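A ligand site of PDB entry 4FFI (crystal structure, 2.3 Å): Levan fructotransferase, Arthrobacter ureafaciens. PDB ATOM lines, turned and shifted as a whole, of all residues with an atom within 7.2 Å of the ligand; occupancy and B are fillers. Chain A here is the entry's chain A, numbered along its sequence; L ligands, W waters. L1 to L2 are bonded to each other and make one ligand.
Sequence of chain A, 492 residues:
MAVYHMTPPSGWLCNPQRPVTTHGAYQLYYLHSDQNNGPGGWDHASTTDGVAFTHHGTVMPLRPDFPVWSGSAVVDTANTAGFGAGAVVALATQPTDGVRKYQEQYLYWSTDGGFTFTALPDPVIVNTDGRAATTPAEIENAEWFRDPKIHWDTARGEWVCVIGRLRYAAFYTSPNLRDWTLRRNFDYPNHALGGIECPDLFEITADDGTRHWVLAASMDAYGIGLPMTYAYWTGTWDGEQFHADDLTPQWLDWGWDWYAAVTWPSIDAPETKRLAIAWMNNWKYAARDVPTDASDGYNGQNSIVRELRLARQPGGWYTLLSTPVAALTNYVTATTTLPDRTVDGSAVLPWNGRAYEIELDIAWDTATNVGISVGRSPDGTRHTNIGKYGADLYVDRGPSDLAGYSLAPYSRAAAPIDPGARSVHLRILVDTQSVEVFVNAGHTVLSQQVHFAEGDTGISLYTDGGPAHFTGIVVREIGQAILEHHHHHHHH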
ATOM      1  N   THR A 128      30.332  -5.307  10.564  1.00  0.00           N
ATOM      2  CA  THR A 128      31.389  -4.447  10.081  1.00  0.00           C
ATOM      3  C   THR A 128      30.847  -3.173   9.442  1.00  0.00           C
ATOM      4  O   THR A 128      31.339  -2.074   9.701  1.00  0.00           O
ATOM      5  CB  THR A 128      32.274  -5.187   9.085  1.00  0.00           C
ATOM      6  OG1 THR A 128      31.453  -5.843   8.107  1.00  0.00           O
ATOM      7  CG2 THR A 128      33.138  -6.220   9.798  1.00  0.00           C
ATOM      8  N   ASP A 129      29.828  -3.322   8.599  1.00  0.00           N
ATOM      9  CA  ASP A 129      29.224  -2.183   7.917  1.00  0.00           C
ATOM     10  C   ASP A 129      28.858  -1.068   8.875  1.00  0.00           C
ATOM     11  O   ASP A 129      29.046   0.110   8.579  1.00  0.00           O
ATOM     12  CB  ASP A 129      27.956  -2.622   7.160  1.00  0.00           C
ATOM     13  CG  ASP A 129      28.265  -3.515   5.973  1.00  0.00           C
ATOM     14  OD1 ASP A 129      27.299  -3.953   5.304  1.00  0.00           O
ATOM     15  OD2 ASP A 129      29.454  -3.772   5.704  1.00  0.00           O
ATOM     16  N   ALA A 137      22.359   6.191   3.922  1.00  0.00           N
ATOM     17  CA  ALA A 137      22.044   4.961   3.213  1.00  0.00           C
ATOM     18  C   ALA A 137      22.783   3.802   3.868  1.00  0.00           C
ATOM     19  O   ALA A 137      22.234   2.708   4.034  1.00  0.00           O
ATOM     20  CB  ALA A 137      22.440   5.086   1.748  1.00  0.00           C
ATOM     21  N   ASN A 141      21.375   0.442   6.074  1.00  0.00           N
ATOM     22  CA  ASN A 141      21.776  -0.903   5.707  1.00  0.00           C
ATOM     23  C   ASN A 141      22.353  -1.604   6.927  1.00  0.00           C
ATOM     24  O   ASN A 141      22.074  -2.778   7.176  1.00  0.00           O
ATOM     25  CB  ASN A 141      22.828  -0.867   4.599  1.00  0.00           C
ATOM     26  CG  ASN A 141      23.326  -2.249   4.202  1.00  0.00           C
ATOM     27  OD1 ASN A 141      22.523  -3.130   3.901  1.00  0.00           O
ATOM     28  ND2 ASN A 141      24.638  -2.443   4.209  1.00  0.00           N
ATOM     29  N   ALA A 142      23.150  -0.874   7.692  1.00  0.00           N
ATOM     30  CA  ALA A 142      23.778  -1.423   8.890  1.00  0.00           C
ATOM     31  C   ALA A 142      22.758  -1.703   9.981  1.00  0.00           C
ATOM     32  O   ALA A 142      23.035  -2.448  10.909  1.00  0.00           O
ATOM     33  CB  ALA A 142      24.843  -0.470   9.406  1.00  0.00           C
ATOM     34  N   PHE A 145      20.529  -6.226   9.857  1.00  0.00           N
ATOM     35  CA  PHE A 145      21.474  -7.325   9.786  1.00  0.00           C
ATOM     36  C   PHE A 145      21.075  -8.214  10.969  1.00  0.00           C
ATOM     37  O   PHE A 145      21.795  -8.310  11.966  1.00  0.00           O
ATOM     38  CB  PHE A 145      22.890  -6.775   9.977  1.00  0.00           C
ATOM     39  CG  PHE A 145      23.974  -7.803   9.905  1.00  0.00           C
ATOM     40  CD1 PHE A 145      24.108  -8.609   8.773  1.00  0.00           C
ATOM     41  CD2 PHE A 145      24.879  -7.955  10.953  1.00  0.00           C
ATOM     42  CE1 PHE A 145      25.122  -9.552   8.705  1.00  0.00           C
ATOM     43  CE2 PHE A 145      25.893  -8.898  10.885  1.00  0.00           C
ATOM     44  CZ  PHE A 145      26.010  -9.702   9.758  1.00  0.00           C
ATOM     45  N   ARG A 165      18.593  -8.868   5.737  1.00  0.00           N
ATOM     46  CA  ARG A 165      19.111  -7.533   5.490  1.00  0.00           C
ATOM     47  C   ARG A 165      18.021  -6.726   4.797  1.00  0.00           C
ATOM     48  O   ARG A 165      16.931  -7.238   4.575  1.00  0.00           O
ATOM     49  CB  ARG A 165      20.340  -7.615   4.592  1.00  0.00           C
ATOM     50  CG  ARG A 165      21.547  -8.213   5.286  1.00  0.00           C
ATOM     51  CD  ARG A 165      22.282  -7.136   6.057  1.00  0.00           C
ATOM     52  NE  ARG A 165      23.696  -7.114   5.700  1.00  0.00           N
ATOM     53  CZ  ARG A 165      24.518  -6.113   5.966  1.00  0.00           C
ATOM     54  NH1 ARG A 165      24.081  -5.044   6.588  1.00  0.00           N
ATOM     55  NH2 ARG A 165      25.783  -6.189   5.585  1.00  0.00           N
ATOM     56  N   LEU A 166      18.314  -5.478   4.446  1.00  0.00           N
ATOM     57  CA  LEU A 166      17.316  -4.639   3.771  1.00  0.00           C
ATOM     58  C   LEU A 166      17.111  -5.051   2.323  1.00  0.00           C
ATOM     59  O   LEU A 166      17.964  -4.817   1.463  1.00  0.00           O
ATOM     60  CB  LEU A 166      17.710  -3.168   3.844  1.00  0.00           C
ATOM     61  CG  LEU A 166      16.807  -2.179   3.092  1.00  0.00           C
ATOM     62  CD1 LEU A 166      15.388  -2.222   3.645  1.00  0.00           C
ATOM     63  CD2 LEU A 166      17.392  -0.779   3.221  1.00  0.00           C
ATOM     64  N   ARG A 167      15.955  -5.668   2.054  1.00  0.00           N
ATOM     65  CA  ARG A 167      15.588  -6.116   0.722  1.00  0.00           C
ATOM     66  C   ARG A 167      16.536  -7.133   0.115  1.00  0.00           C
ATOM     67  O   ARG A 167      16.663  -7.231  -1.101  1.00  0.00           O
ATOM     68  CB  ARG A 167      15.408  -4.913  -0.204  1.00  0.00           C
ATOM     69  CG  ARG A 167      14.367  -3.911   0.292  1.00  0.00           C
ATOM     70  CD  ARG A 167      12.975  -4.531   0.396  1.00  0.00           C
ATOM     71  NE  ARG A 167      11.980  -3.607   0.934  1.00  0.00           N
ATOM     72  CZ  ARG A 167      11.799  -3.349   2.226  1.00  0.00           C
ATOM     73  NH1 ARG A 167      12.533  -3.949   3.140  1.00  0.00           N
ATOM     74  NH2 ARG A 167      10.880  -2.463   2.599  1.00  0.00           N
ATOM     75  N   TYR A 168      17.223  -7.895   0.964  1.00  0.00           N
ATOM     76  CA  TYR A 168      18.126  -8.941   0.504  1.00  0.00           C
ATOM     77  C   TYR A 168      18.563  -9.775   1.699  1.00  0.00           C
ATOM     78  O   TYR A 168      18.289  -9.403   2.839  1.00  0.00           O
ATOM     79  CB  TYR A 168      19.328  -8.342  -0.249  1.00  0.00           C
ATOM     80  CG  TYR A 168      20.394  -7.672   0.589  1.00  0.00           C
ATOM     81  CD1 TYR A 168      21.511  -8.372   1.026  1.00  0.00           C
ATOM     82  CD2 TYR A 168      20.296  -6.321   0.917  1.00  0.00           C
ATOM     83  CE1 TYR A 168      22.517  -7.742   1.772  1.00  0.00           C
ATOM     84  CE2 TYR A 168      21.283  -5.682   1.656  1.00  0.00           C
ATOM     85  CZ  TYR A 168      22.396  -6.389   2.081  1.00  0.00           C
ATOM     86  OH  TYR A 168      23.373  -5.762   2.814  1.00  0.00           O
ATOM     87  N   ALA A 169      19.223 -10.902   1.447  1.00  0.00           N
ATOM     88  CA  ALA A 169      19.680 -11.777   2.516  1.00  0.00           C
ATOM     89  C   ALA A 169      21.145 -12.166   2.364  1.00  0.00           C
ATOM     90  O   ALA A 169      21.622 -12.354   1.260  1.00  0.00           O
ATOM     91  CB  ALA A 169      18.821 -13.026   2.559  1.00  0.00           C
ATOM     92  N   ALA A 170      21.846 -12.292   3.492  1.00  0.00           N
ATOM     93  CA  ALA A 170      23.269 -12.646   3.478  1.00  0.00           C
ATOM     94  C   ALA A 170      23.521 -14.063   3.974  1.00  0.00           C
ATOM     95  O   ALA A 170      22.792 -14.572   4.828  1.00  0.00           O
ATOM     96  CB  ALA A 170      24.070 -11.642   4.315  1.00  0.00           C
ATOM     97  N   PHE A 171      24.566 -14.701   3.454  1.00  0.00           N
ATOM     98  CA  PHE A 171      24.908 -16.059   3.847  1.00  0.00           C
ATOM     99  C   PHE A 171      26.331 -16.191   4.383  1.00  0.00           C
ATOM    100  O   PHE A 171      27.252 -15.503   3.945  1.00  0.00           O
ATOM    101  CB  PHE A 171      24.740 -17.018   2.680  1.00  0.00           C
ATOM    102  CG  PHE A 171      23.302 -17.202   2.256  1.00  0.00           C
ATOM    103  CD1 PHE A 171      22.622 -16.191   1.600  1.00  0.00           C
ATOM    104  CD2 PHE A 171      22.645 -18.402   2.522  1.00  0.00           C
ATOM    105  CE1 PHE A 171      21.300 -16.345   1.212  1.00  0.00           C
ATOM    106  CE2 PHE A 171      21.313 -18.571   2.144  1.00  0.00           C
ATOM    107  CZ  PHE A 171      20.638 -17.552   1.484  1.00  0.00           C
ATOM    108  N   TYR A 172      26.486 -17.101   5.339  1.00  0.00           N
ATOM    109  CA  TYR A 172      27.762 -17.392   5.983  1.00  0.00           C
ATOM    110  C   TYR A 172      27.891 -18.894   6.249  1.00  0.00           C
ATOM    111  O   TYR A 172      26.910 -19.577   6.521  1.00  0.00           O
ATOM    112  CB  TYR A 172      27.876 -16.654   7.325  1.00  0.00           C
ATOM    113  CG  TYR A 172      27.863 -15.149   7.251  1.00  0.00           C
ATOM    114  CD1 TYR A 172      26.692 -14.442   6.979  1.00  0.00           C
ATOM    115  CD2 TYR A 172      29.030 -14.411   7.478  1.00  0.00           C
ATOM    116  CE1 TYR A 172      26.678 -13.044   6.937  1.00  0.00           C
ATOM    117  CE2 TYR A 172      29.019 -13.021   7.448  1.00  0.00           C
ATOM    118  CZ  TYR A 172      27.845 -12.342   7.175  1.00  0.00           C
ATOM    119  OH  TYR A 172      27.849 -10.968   7.139  1.00  0.00           O
ATOM    120  N   LEU A 182      31.941 -15.172   5.149  1.00  0.00           N
ATOM    121  CA  LEU A 182      30.923 -14.539   4.323  1.00  0.00           C
ATOM    122  C   LEU A 182      30.784 -15.122   2.909  1.00  0.00           C
ATOM    123  O   LEU A 182      31.776 -15.315   2.207  1.00  0.00           O
ATOM    124  CB  LEU A 182      31.199 -13.035   4.227  1.00  0.00           C
ATOM    125  CG  LEU A 182      30.254 -12.195   3.359  1.00  0.00           C
ATOM    126  CD1 LEU A 182      28.842 -12.252   3.900  1.00  0.00           C
ATOM    127  CD2 LEU A 182      30.736 -10.751   3.349  1.00  0.00           C
ATOM    128  N   ARG A 183      29.554 -15.393   2.500  1.00  0.00           N
ATOM    129  CA  ARG A 183      29.301 -15.924   1.173  1.00  0.00           C
ATOM    130  C   ARG A 183      28.550 -14.899   0.334  1.00  0.00           C
ATOM    131  O   ARG A 183      28.467 -13.730   0.709  1.00  0.00           O
ATOM    132  CB  ARG A 183      28.499 -17.224   1.265  1.00  0.00           C
ATOM    133  CG  ARG A 183      29.270 -18.352   1.917  1.00  0.00           C
ATOM    134  CD  ARG A 183      30.634 -18.535   1.268  1.00  0.00           C
ATOM    135  NE  ARG A 183      31.386 -19.644   1.867  1.00  0.00           N
ATOM    136  CZ  ARG A 183      32.666 -19.883   1.633  1.00  0.00           C
ATOM    137  NH1 ARG A 183      33.356 -19.101   0.825  1.00  0.00           N
ATOM    138  NH2 ARG A 183      33.269 -20.920   2.220  1.00  0.00           N
ATOM    139  N   ARG A 184      28.004 -15.329  -0.789  1.00  0.00           N
ATOM    140  CA  ARG A 184      27.290 -14.413  -1.675  1.00  0.00           C
ATOM    141  C   ARG A 184      25.851 -14.200  -1.232  1.00  0.00           C
ATOM    142  O   ARG A 184      25.210 -15.099  -0.696  1.00  0.00           O
ATOM    143  CB  ARG A 184      27.357 -14.931  -3.110  1.00  0.00           C
ATOM    144  CG  ARG A 184      28.795 -15.251  -3.521  1.00  0.00           C
ATOM    145  CD  ARG A 184      28.940 -15.735  -4.967  1.00  0.00           C
ATOM    146  NE  ARG A 184      28.657 -14.676  -5.932  1.00  0.00           N
ATOM    147  CZ  ARG A 184      28.892 -14.775  -7.234  1.00  0.00           C
ATOM    148  NH1 ARG A 184      29.413 -15.893  -7.743  1.00  0.00           N
ATOM    149  NH2 ARG A 184      28.590 -13.769  -8.040  1.00  0.00           N
ATOM    150  N   ASN A 185      25.351 -12.988  -1.454  1.00  0.00           N
ATOM    151  CA  ASN A 185      23.983 -12.646  -1.078  1.00  0.00           C
ATOM    152  C   ASN A 185      22.942 -13.238  -1.982  1.00  0.00           C
ATOM    153  O   ASN A 185      23.239 -13.779  -3.049  1.00  0.00           O
ATOM    154  CB  ASN A 185      23.778 -11.137  -1.088  1.00  0.00           C
ATOM    155  CG  ASN A 185      24.682 -10.418  -0.137  1.00  0.00           C
ATOM    156  OD1 ASN A 185      25.033 -10.947   0.911  1.00  0.00           O
ATOM    157  ND2 ASN A 185      25.047  -9.192  -0.485  1.00  0.00           N
ATOM    158  N   PHE A 186      21.697 -13.131  -1.541  1.00  0.00           N
ATOM    159  CA  PHE A 186      20.581 -13.592  -2.330  1.00  0.00           C
ATOM    160  C   PHE A 186      19.791 -12.339  -2.650  1.00  0.00           C
ATOM    161  O   PHE A 186      19.325 -11.654  -1.751  1.00  0.00           O
ATOM    162  CB  PHE A 186      19.688 -14.544  -1.539  1.00  0.00           C
ATOM    163  CG  PHE A 186      18.417 -14.878  -2.259  1.00  0.00           C
ATOM    164  CD1 PHE A 186      18.447 -15.636  -3.430  1.00  0.00           C
ATOM    165  CD2 PHE A 186      17.216 -14.363  -1.821  1.00  0.00           C
ATOM    166  CE1 PHE A 186      17.286 -15.853  -4.157  1.00  0.00           C
ATOM    167  CE2 PHE A 186      16.047 -14.579  -2.537  1.00  0.00           C
ATOM    168  CZ  PHE A 186      16.078 -15.323  -3.708  1.00  0.00           C
ATOM    169  N   ASP A 187      19.678 -12.026  -3.933  1.00  0.00           N
ATOM    170  CA  ASP A 187      18.918 -10.845  -4.334  1.00  0.00           C
ATOM    171  C   ASP A 187      17.697 -11.303  -5.089  1.00  0.00           C
ATOM    172  O   ASP A 187      17.683 -12.377  -5.664  1.00  0.00           O
ATOM    173  CB  ASP A 187      19.747  -9.925  -5.228  1.00  0.00           C
ATOM    174  CG  ASP A 187      20.834  -9.183  -4.468  1.00  0.00           C
ATOM    175  OD1 ASP A 187      22.010  -9.579  -4.551  1.00  0.00           O
ATOM    176  OD2 ASP A 187      20.501  -8.183  -3.794  1.00  0.00           O
ATOM    177  N   HIS A 191      11.503  -5.664  -5.110  1.00  0.00           N
ATOM    178  CA  HIS A 191      11.728  -5.123  -3.778  1.00  0.00           C
ATOM    179  C   HIS A 191      10.479  -4.611  -3.089  1.00  0.00           C
ATOM    180  O   HIS A 191      10.491  -4.299  -1.899  1.00  0.00           O
ATOM    181  CB  HIS A 191      12.782  -4.014  -3.831  1.00  0.00           C
ATOM    182  CG  HIS A 191      14.171  -4.530  -3.974  1.00  0.00           C
ATOM    183  ND1 HIS A 191      15.277  -3.716  -3.899  1.00  0.00           N
ATOM    184  CD2 HIS A 191      14.645  -5.790  -4.160  1.00  0.00           C
ATOM    185  CE1 HIS A 191      16.375  -4.452  -4.037  1.00  0.00           C
ATOM    186  NE2 HIS A 191      16.021  -5.704  -4.187  1.00  0.00           N
HETATM  187  C1  LIG L   1      27.422  -8.619   2.301  1.00  0.00           C
HETATM  188  C2  LIG L   1      27.683  -7.274   1.702  1.00  0.00           C
HETATM  189  C3  LIG L   1      27.268  -6.145   2.594  1.00  0.00           C
HETATM  190  C4  LIG L   1      26.975  -5.100   1.640  1.00  0.00           C
HETATM  191  C5  LIG L   1      26.159  -5.914   0.709  1.00  0.00           C
HETATM  192  C6  LIG L   1      25.714  -5.275  -0.574  1.00  0.00           C
HETATM  193  O1  LIG L   1      26.104  -8.938   2.523  1.00  0.00           O
HETATM  194  O2  LIG L   1      29.015  -7.145   1.384  1.00  0.00           O
HETATM  195  O3  LIG L   1      28.241  -5.780   3.499  1.00  0.00           O
HETATM  196  O4  LIG L   1      26.165  -4.147   2.241  1.00  0.00           O
HETATM  197  O5  LIG L   1      26.909  -7.095   0.513  1.00  0.00           O
HETATM  198  O6  LIG L   1      25.548  -6.107  -1.690  1.00  0.00           O
HETATM  199  C1  LG2 L   2      25.917  -5.731  -3.977  1.00  0.00           C
HETATM  200  C2  LG2 L   2      24.948  -5.578  -2.829  1.00  0.00           C
HETATM  201  C3  LG2 L   2      23.641  -6.227  -3.172  1.00  0.00           C
HETATM  202  C4  LG2 L   2      22.771  -5.601  -2.213  1.00  0.00           C
HETATM  203  C5  LG2 L   2      23.223  -4.188  -2.254  1.00  0.00           C
HETATM  204  C6  LG2 L   2      22.916  -3.432  -0.996  1.00  0.00           C
HETATM  205  O1  LG2 L   2      25.679  -5.018  -5.134  1.00  0.00           O
HETATM  206  O2  LG2 L   2      23.660  -7.590  -3.083  1.00  0.00           O
HETATM  207  O3  LG2 L   2      21.463  -5.633  -2.695  1.00  0.00           O
HETATM  208  O4  LG2 L   2      24.603  -4.221  -2.563  1.00  0.00           O
HETATM  209  O5  LG2 L   2      23.178  -2.073  -0.970  1.00  0.00           O
HETATM  210  O   HOH W   1      26.710  -9.480   5.415  1.00  0.00           O
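ND2 of Asn 141 lies within hydrogen-bond range of OD1 of Asp 129 (3.2 Å).
The guanidinium group of Arg 165 lies within salt-bridge range of the side-chain carboxylate of Asp 129.
O of Asn 141 is in hydrogen-bond range of NH1 of Arg 165.
OD1 of Asn 141 lies within hydrogen-bond range of OH of Tyr 168, at 3.0 Å.
NE of Arg 165 is in hydrogen-bond range of OH of Tyr 168, at 3.2 Å.
The side-chain carboxylate (OD1) of Asp 129 is in hydrogen-bond range of an oxygen (O3) of LIG L1, 2.7 Å away.
The side-chain amide oxygen (OD1) of Asn 185 sits at hydrogen-bond distance from an oxygen (O1) of LIG L1 (2.8 Å).
The side-chain carboxylate (OD2) of Asp 187 lies within hydrogen-bond range of an oxygen (O3) of LG2 L2, at 2.9 Å.
The side-chain amide nitrogen of Asn 141 lies within hydrogen-bond range of an oxygen (O4) of LIG L1, 3.0 Å away.
NH2 of Arg 165 is in hydrogen-bond range of O3 of LIG L1 (3.2 Å).
The side-chain hydroxyl of Tyr 168 is in hydrogen-bond range of an oxygen (O4) of LIG L1, at 3.3 Å.
Water W1 lies within hydrogen-bond range of OH of Tyr 172, O1 of LIG L1 and NH2 of Arg 165.
CB of Ala 170 touches O1 of LIG L1, 3.8 Å away.
Hydrophobic or aromatic side chains that line the ligand: Tyr 168 and Ala 170.
Within 4 Å of the ligand: Asp 129, Asn 141, Arg 165, Tyr 168, Ala 170, Asn 185 and Asp 187.
The nearest printed residue that does not touch the ligand is Leu 182 (4.1 Å).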
